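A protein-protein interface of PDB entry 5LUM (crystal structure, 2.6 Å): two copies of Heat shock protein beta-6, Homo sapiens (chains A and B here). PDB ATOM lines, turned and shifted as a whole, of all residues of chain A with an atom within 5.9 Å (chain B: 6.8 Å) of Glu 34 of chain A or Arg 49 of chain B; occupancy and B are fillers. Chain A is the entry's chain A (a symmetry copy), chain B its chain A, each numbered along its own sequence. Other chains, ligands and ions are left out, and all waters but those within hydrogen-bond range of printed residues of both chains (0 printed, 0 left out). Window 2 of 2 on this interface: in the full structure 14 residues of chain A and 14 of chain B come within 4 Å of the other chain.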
ATOM      1  N   HIS A  32      18.521  34.982 -10.789  1.00  0.00           N
ATOM      2  CA  HIS A  32      18.793  34.125 -11.940  1.00  0.00           C
ATOM      3  C   HIS A  32      18.233  32.760 -11.677  1.00  0.00           C
ATOM      4  O   HIS A  32      18.395  32.218 -10.584  1.00  0.00           O
ATOM      5  CB  HIS A  32      20.267  34.091 -12.411  1.00  0.00           C
ATOM      6  CG  HIS A  32      21.228  33.288 -11.591  1.00  0.00           C
ATOM      7  ND1 HIS A  32      21.180  31.902 -11.563  1.00  0.00           N
ATOM      8  CD2 HIS A  32      22.331  33.699 -10.922  1.00  0.00           C
ATOM      9  CE1 HIS A  32      22.218  31.520 -10.834  1.00  0.00           C
ATOM     10  NE2 HIS A  32      22.923  32.572 -10.400  1.00  0.00           N
ATOM     11  N   GLU A  33      17.547  32.220 -12.668  1.00  0.00           N
ATOM     12  CA  GLU A  33      16.997  30.877 -12.591  1.00  0.00           C
ATOM     13  C   GLU A  33      18.103  29.827 -12.569  1.00  0.00           C
ATOM     14  O   GLU A  33      19.250  30.145 -12.830  1.00  0.00           O
ATOM     15  CB  GLU A  33      16.011  30.639 -13.735  1.00  0.00           C
ATOM     16  CG  GLU A  33      14.732  30.044 -13.175  1.00  0.00           C
ATOM     17  CD  GLU A  33      13.465  30.721 -13.644  1.00  0.00           C
ATOM     18  OE1 GLU A  33      13.388  31.090 -14.840  1.00  0.00           O
ATOM     19  OE2 GLU A  33      12.525  30.827 -12.824  1.00  0.00           O
ATOM     20  N   GLU A  34      17.770  28.592 -12.191  1.00  0.00           N
ATOM     21  CA  GLU A  34      18.728  27.488 -12.047  1.00  0.00           C
ATOM     22  C   GLU A  34      19.624  27.260 -13.270  1.00  0.00           C
ATOM     23  O   GLU A  34      19.141  27.126 -14.407  1.00  0.00           O
ATOM     24  CB  GLU A  34      17.976  26.241 -11.663  1.00  0.00           C
ATOM     25  CG  GLU A  34      18.853  25.035 -11.534  1.00  0.00           C
ATOM     26  CD  GLU A  34      18.175  23.995 -10.693  1.00  0.00           C
ATOM     27  OE1 GLU A  34      17.551  23.089 -11.286  1.00  0.00           O
ATOM     28  OE2 GLU A  34      18.198  24.131  -9.447  1.00  0.00           O
ATOM     29  N   ARG A  35      20.939  27.229 -13.021  1.00  0.00           N
ATOM     30  CA  ARG A  35      21.927  27.047 -14.073  1.00  0.00           C
ATOM     31  C   ARG A  35      23.050  26.075 -13.691  1.00  0.00           C
ATOM     32  O   ARG A  35      23.313  25.848 -12.525  1.00  0.00           O
ATOM     33  CB  ARG A  35      22.456  28.385 -14.578  1.00  0.00           C
ATOM     34  CG  ARG A  35      23.181  29.257 -13.623  1.00  0.00           C
ATOM     35  CD  ARG A  35      23.814  30.329 -14.460  1.00  0.00           C
ATOM     36  NE  ARG A  35      23.024  31.558 -14.632  1.00  0.00           N
ATOM     37  CZ  ARG A  35      23.514  32.773 -14.352  1.00  0.00           C
ATOM     38  NH1 ARG A  35      24.744  32.906 -13.866  1.00  0.00           N
ATOM     39  NH2 ARG A  35      22.782  33.859 -14.566  1.00  0.00           N
ATOM     40  N   PRO A  36      23.632  25.364 -14.671  1.00  0.00           N
ATOM     41  CA  PRO A  36      24.599  24.310 -14.323  1.00  0.00           C
ATOM     42  C   PRO A  36      25.961  24.823 -13.887  1.00  0.00           C
ATOM     43  O   PRO A  36      26.362  25.934 -14.279  1.00  0.00           O
ATOM     44  CB  PRO A  36      24.685  23.524 -15.621  1.00  0.00           C
ATOM     45  CG  PRO A  36      24.479  24.552 -16.667  1.00  0.00           C
ATOM     46  CD  PRO A  36      23.417  25.421 -16.140  1.00  0.00           C
ATOM     47  N   HIS A  39      29.754  21.345  -9.997  1.00  0.00           N
ATOM     48  CA  HIS A  39      29.287  20.190  -9.225  1.00  0.00           C
ATOM     49  C   HIS A  39      27.794  19.878  -9.319  1.00  0.00           C
ATOM     50  O   HIS A  39      27.432  18.690  -9.215  1.00  0.00           O
ATOM     51  CB  HIS A  39      29.718  20.318  -7.767  1.00  0.00           C
ATOM     52  CG  HIS A  39      31.205  20.274  -7.612  1.00  0.00           C
ATOM     53  ND1 HIS A  39      31.956  21.436  -7.515  1.00  0.00           N
ATOM     54  CD2 HIS A  39      32.041  19.206  -7.588  1.00  0.00           C
ATOM     55  CE1 HIS A  39      33.219  21.039  -7.437  1.00  0.00           C
ATOM     56  NE2 HIS A  39      33.322  19.705  -7.472  1.00  0.00           N
ATOM     57  N   GLY A  40      26.955  20.891  -9.523  1.00  0.00           N
ATOM     58  CA  GLY A  40      25.513  20.672  -9.632  1.00  0.00           C
ATOM     59  C   GLY A  40      24.775  21.743 -10.415  1.00  0.00           C
ATOM     60  O   GLY A  40      25.189  22.131 -11.508  1.00  0.00           O
ATOM     61  N   PHE A  41      23.670  22.229  -9.851  1.00  0.00           N
ATOM     62  CA  PHE A  41      22.907  23.363 -10.395  1.00  0.00           C
ATOM     63  C   PHE A  41      22.908  24.425  -9.320  1.00  0.00           C
ATOM     64  O   PHE A  41      23.061  24.102  -8.143  1.00  0.00           O
ATOM     65  CB  PHE A  41      21.457  22.969 -10.717  1.00  0.00           C
ATOM     66  CG  PHE A  41      21.293  22.018 -11.877  1.00  0.00           C
ATOM     67  CD1 PHE A  41      21.282  22.491 -13.187  1.00  0.00           C
ATOM     68  CD2 PHE A  41      21.202  20.645 -11.665  1.00  0.00           C
ATOM     69  CE1 PHE A  41      21.170  21.616 -14.260  1.00  0.00           C
ATOM     70  CE2 PHE A  41      21.072  19.767 -12.741  1.00  0.00           C
ATOM     71  CZ  PHE A  41      21.030  20.262 -14.029  1.00  0.00           C
ATOM     72  N   VAL A  42      22.794  25.685  -9.724  1.00  0.00           N
ATOM     73  CA  VAL A  42      22.737  26.827  -8.800  1.00  0.00           C
ATOM     74  C   VAL A  42      21.828  27.946  -9.365  1.00  0.00           C
ATOM     75  O   VAL A  42      21.946  28.313 -10.532  1.00  0.00           O
ATOM     76  CB  VAL A  42      24.165  27.343  -8.448  1.00  0.00           C
ATOM     77  CG1 VAL A  42      24.942  27.747  -9.729  1.00  0.00           C
ATOM     78  CG2 VAL A  42      24.122  28.472  -7.421  1.00  0.00           C
ATOM     79  N   ALA A  43      20.913  28.430  -8.516  1.00  0.00           N
ATOM     80  CA  ALA A  43      19.971  29.556  -8.666  1.00  0.00           C
ATOM     81  C   ALA A  43      20.301  30.503  -7.507  1.00  0.00           C
ATOM     82  O   ALA A  43      20.612  30.060  -6.400  1.00  0.00           O
ATOM     83  CB  ALA A  43      18.527  29.086  -8.547  1.00  0.00           C
ATOM     84  N   VAL B  22      15.598  15.200  -2.170  1.00  0.00           N
ATOM     85  CA  VAL B  22      14.374  15.188  -2.969  1.00  0.00           C
ATOM     86  C   VAL B  22      14.673  14.380  -4.236  1.00  0.00           C
ATOM     87  O   VAL B  22      15.419  14.827  -5.119  1.00  0.00           O
ATOM     88  CB  VAL B  22      13.841  16.606  -3.329  1.00  0.00           C
ATOM     89  CG1 VAL B  22      12.482  16.531  -4.025  1.00  0.00           C
ATOM     90  CG2 VAL B  22      13.763  17.503  -2.099  1.00  0.00           C
ATOM     91  N   HIS B  25      18.215  13.792  -5.993  1.00  0.00           N
ATOM     92  CA  HIS B  25      19.014  14.970  -5.697  1.00  0.00           C
ATOM     93  C   HIS B  25      19.071  15.361  -4.220  1.00  0.00           C
ATOM     94  O   HIS B  25      18.135  15.100  -3.461  1.00  0.00           O
ATOM     95  CB  HIS B  25      18.489  16.164  -6.494  1.00  0.00           C
ATOM     96  CG  HIS B  25      18.863  16.112  -7.943  1.00  0.00           C
ATOM     97  ND1 HIS B  25      18.098  15.397  -8.866  1.00  0.00           N
ATOM     98  CD2 HIS B  25      19.918  16.665  -8.584  1.00  0.00           C
ATOM     99  CE1 HIS B  25      18.731  15.522 -10.022  1.00  0.00           C
ATOM    100  NE2 HIS B  25      19.825  16.282  -9.905  1.00  0.00           N
ATOM    101  N   VAL B  26      20.182  16.039  -3.845  1.00  0.00           N
ATOM    102  CA  VAL B  26      20.399  16.678  -2.562  1.00  0.00           C
ATOM    103  C   VAL B  26      20.222  18.172  -2.842  1.00  0.00           C
ATOM    104  O   VAL B  26      20.898  18.716  -3.733  1.00  0.00           O
ATOM    105  CB  VAL B  26      21.786  16.376  -1.957  1.00  0.00           C
ATOM    106  CG1 VAL B  26      21.993  17.165  -0.662  1.00  0.00           C
ATOM    107  CG2 VAL B  26      21.955  14.885  -1.711  1.00  0.00           C
ATOM    108  N   GLU B  27      19.282  18.816  -2.145  1.00  0.00           N
ATOM    109  CA  GLU B  27      19.014  20.238  -2.317  1.00  0.00           C
ATOM    110  C   GLU B  27      19.504  21.006  -1.129  1.00  0.00           C
ATOM    111  O   GLU B  27      19.337  20.553   0.001  1.00  0.00           O
ATOM    112  CB  GLU B  27      17.512  20.501  -2.532  1.00  0.00           C
ATOM    113  CG  GLU B  27      16.928  19.830  -3.764  1.00  0.00           C
ATOM    114  CD  GLU B  27      15.545  20.300  -4.172  1.00  0.00           C
ATOM    115  OE1 GLU B  27      14.878  21.031  -3.404  1.00  0.00           O
ATOM    116  OE2 GLU B  27      15.120  19.925  -5.281  1.00  0.00           O
ATOM    117  N   VAL B  28      20.102  22.174  -1.376  1.00  0.00           N
ATOM    118  CA  VAL B  28      20.506  23.139  -0.351  1.00  0.00           C
ATOM    119  C   VAL B  28      19.775  24.446  -0.651  1.00  0.00           C
ATOM    120  O   VAL B  28      19.853  24.976  -1.766  1.00  0.00           O
ATOM    121  CB  VAL B  28      22.022  23.349  -0.267  1.00  0.00           C
ATOM    122  CG1 VAL B  28      22.365  24.277   0.890  1.00  0.00           C
ATOM    123  CG2 VAL B  28      22.743  22.018  -0.125  1.00  0.00           C
ATOM    124  N   HIS B  29      19.018  24.916   0.334  1.00  0.00           N
ATOM    125  CA  HIS B  29      18.246  26.143   0.253  1.00  0.00           C
ATOM    126  C   HIS B  29      18.717  27.044   1.368  1.00  0.00           C
ATOM    127  O   HIS B  29      18.587  26.679   2.535  1.00  0.00           O
ATOM    128  CB  HIS B  29      16.731  25.846   0.346  1.00  0.00           C
ATOM    129  CG  HIS B  29      16.229  24.913  -0.721  1.00  0.00           C
ATOM    130  ND1 HIS B  29      16.103  25.319  -2.039  1.00  0.00           N
ATOM    131  CD2 HIS B  29      15.828  23.622  -0.621  1.00  0.00           C
ATOM    132  CE1 HIS B  29      15.647  24.267  -2.698  1.00  0.00           C
ATOM    133  NE2 HIS B  29      15.445  23.230  -1.883  1.00  0.00           N
ATOM    134  N   HIS B  47      19.725  28.467  -4.021  1.00  0.00           N
ATOM    135  CA  HIS B  47      19.219  27.111  -4.149  1.00  0.00           C
ATOM    136  C   HIS B  47      20.253  26.354  -4.962  1.00  0.00           C
ATOM    137  O   HIS B  47      20.508  26.723  -6.106  1.00  0.00           O
ATOM    138  CB  HIS B  47      17.863  27.090  -4.892  1.00  0.00           C
ATOM    139  CG  HIS B  47      16.878  28.124  -4.420  1.00  0.00           C
ATOM    140  ND1 HIS B  47      15.787  27.762  -3.648  1.00  0.00           N
ATOM    141  CD2 HIS B  47      16.855  29.478  -4.606  1.00  0.00           C
ATOM    142  CE1 HIS B  47      15.128  28.890  -3.413  1.00  0.00           C
ATOM    143  NE2 HIS B  47      15.747  29.951  -3.951  1.00  0.00           N
ATOM    144  N   ARG B  48      20.882  25.336  -4.376  1.00  0.00           N
ATOM    145  CA  ARG B  48      21.808  24.454  -5.086  1.00  0.00           C
ATOM    146  C   ARG B  48      21.276  23.054  -5.075  1.00  0.00           C
ATOM    147  O   ARG B  48      20.660  22.626  -4.106  1.00  0.00           O
ATOM    148  CB  ARG B  48      23.241  24.519  -4.567  1.00  0.00           C
ATOM    149  CG  ARG B  48      23.774  25.908  -4.764  1.00  0.00           C
ATOM    150  CD  ARG B  48      25.127  26.113  -4.167  1.00  0.00           C
ATOM    151  NE  ARG B  48      26.102  25.498  -5.029  1.00  0.00           N
ATOM    152  CZ  ARG B  48      26.998  26.158  -5.738  1.00  0.00           C
ATOM    153  NH1 ARG B  48      27.097  27.476  -5.629  1.00  0.00           N
ATOM    154  NH2 ARG B  48      27.848  25.501  -6.509  1.00  0.00           N
ATOM    155  N   ARG B  49      21.535  22.328  -6.143  1.00  0.00           N
ATOM    156  CA  ARG B  49      21.064  20.967  -6.323  1.00  0.00           C
ATOM    157  C   ARG B  49      22.212  20.084  -6.824  1.00  0.00           C
ATOM    158  O   ARG B  49      22.933  20.465  -7.737  1.00  0.00           O
ATOM    159  CB  ARG B  49      19.945  21.013  -7.345  1.00  0.00           C
ATOM    160  CG  ARG B  49      18.859  20.023  -7.128  1.00  0.00           C
ATOM    161  CD  ARG B  49      17.578  20.535  -7.757  1.00  0.00           C
ATOM    162  NE  ARG B  49      17.708  20.847  -9.184  1.00  0.00           N
ATOM    163  CZ  ARG B  49      17.531  19.973 -10.161  1.00  0.00           C
ATOM    164  NH1 ARG B  49      17.264  18.709  -9.884  1.00  0.00           N
ATOM    165  NH2 ARG B  49      17.652  20.348 -11.425  1.00  0.00           N
ATOM    166  N   TYR B  50      22.397  18.924  -6.206  1.00  0.00           N
ATOM    167  CA  TYR B  50      23.444  17.973  -6.561  1.00  0.00           C
ATOM    168  C   TYR B  50      22.852  16.606  -6.754  1.00  0.00           C
ATOM    169  O   TYR B  50      22.009  16.226  -5.964  1.00  0.00           O
ATOM    170  CB  TYR B  50      24.444  17.875  -5.430  1.00  0.00           C
ATOM    171  CG  TYR B  50      25.068  19.192  -5.034  1.00  0.00           C
ATOM    172  CD1 TYR B  50      26.200  19.672  -5.688  1.00  0.00           C
ATOM    173  CD2 TYR B  50      24.599  19.904  -3.935  1.00  0.00           C
ATOM    174  CE1 TYR B  50      26.818  20.857  -5.289  1.00  0.00           C
ATOM    175  CE2 TYR B  50      25.209  21.087  -3.529  1.00  0.00           C
ATOM    176  CZ  TYR B  50      26.326  21.550  -4.203  1.00  0.00           C
ATOM    177  OH  TYR B  50      26.980  22.666  -3.773  1.00  0.00           O
ATOM    178  N   ARG B  51      23.313  15.804  -7.719  1.00  0.00           N
ATOM    179  CA  ARG B  51      22.670  14.498  -7.782  1.00  0.00           C
ATOM    180  C   ARG B  51      23.269  13.530  -6.792  1.00  0.00           C
ATOM    181  O   ARG B  51      24.445  13.628  -6.450  1.00  0.00           O
ATOM    182  CB  ARG B  51      22.555  13.917  -9.185  1.00  0.00           C
ATOM    183  CG  ARG B  51      23.661  13.032  -9.643  1.00  0.00           C
ATOM    184  CD  ARG B  51      23.187  12.369 -10.906  1.00  0.00           C
ATOM    185  NE  ARG B  51      23.964  11.182 -11.265  1.00  0.00           N
ATOM    186  CZ  ARG B  51      23.670   9.954 -10.851  1.00  0.00           C
ATOM    187  NH1 ARG B  51      22.652   9.750 -10.009  1.00  0.00           N
ATOM    188  NH2 ARG B  51      24.402   8.925 -11.249  1.00  0.00           N
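No position is printed for both chains. Of the 8 pairs that touch across the chains among the printed residues, none has its exchanged pair printed and touching as well.
Of chain B, only Arg 49 comes within 4 Å of Glu 34 of chain A. Arg 49 of chain B touches just these residues of chain A: Glu 34, Gly 40 and Phe 41. Of the printed residues of chain B, Phe 41 of chain A touches Arg 48 and Arg 49. Printed residues of chain A within 4 Å of His 47 of chain B: Val 42 (3.5 Å) and Ala 43 (3.0 Å). Glu 27 of chain B touches none of the printed residues of chain A. The nearest residue of chain B that does not touch Glu 34 of chain A is His 47 of chain B (4.8 Å). The nearest printed residue of chain A that does not touch Arg 49 of chain B is His 39 of chain A (5.1 Å). The nearest printed residue of chain B that does not touch Val 42 of chain A is Arg 49 of chain B (5.1 Å).
His 39 of chain A touches Tyr 50 of chain B. O of Arg 49 of chain B touches CA of Gly 40 of chain A (3.2 Å). O of Phe 41 of chain A touches CA of Arg 48 of chain B, 3.3 Å away. Val 42 of chain A touches His 47 of chain B (CA to O, 3.5 Å). CG2 of Val 42 of chain A touches NH1 of Arg 48 of chain B (3.6 Å).
The backbone carbonyl oxygen (O) of His 47 of chain B sits at hydrogen-bond distance from the backbone NH (N) of Ala 43 of chain A, 3.0 Å away. OE1 of Glu 34 of chain A lies within salt-bridge range of NH2 of Arg 49 of chain B. N of Phe 41 of chain A is in hydrogen-bond range of O of Arg 49 of chain B, at 2.9 Å.
Of the 11 printed residues of chain B, 4 touch a printed residue of chain A. Hydrophobic or aromatic side chains of chain A within 4 Å of the printed part of chain B: His 39, Phe 41, Val 42 and Ala 43. Among the printed residues, Asp or Glu carboxylates within 4 Å of a Lys or Arg side-chain nitrogen of the other chain: Glu 34 of chain A with Arg 49 of chain B (2.7 Å).
N of Val 26 of chain B sits at hydrogen-bond distance from O of Tyr 50 of chain B. The backbone carbonyl oxygen (O) of Arg 48 of chain B sits at hydrogen-bond distance from the backbone NH (N) of Val 28 of chain B. A ring nitrogen (ND1) of His 29 of chain B sits at hydrogen-bond distance from a ring nitrogen (ND1) of His 47 of chain B, 2.9 Å away. The side-chain hydroxyl (OH) of Tyr 50 of chain B sits at hydrogen-bond distance from the guanidinium group (NE) of Arg 48 of chain B (3.2 Å). The backbone carbonyl oxygen of Arg 35 of chain A is in hydrogen-bond range of the backbone NH of Val 42 of chain A (2.9 Å).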
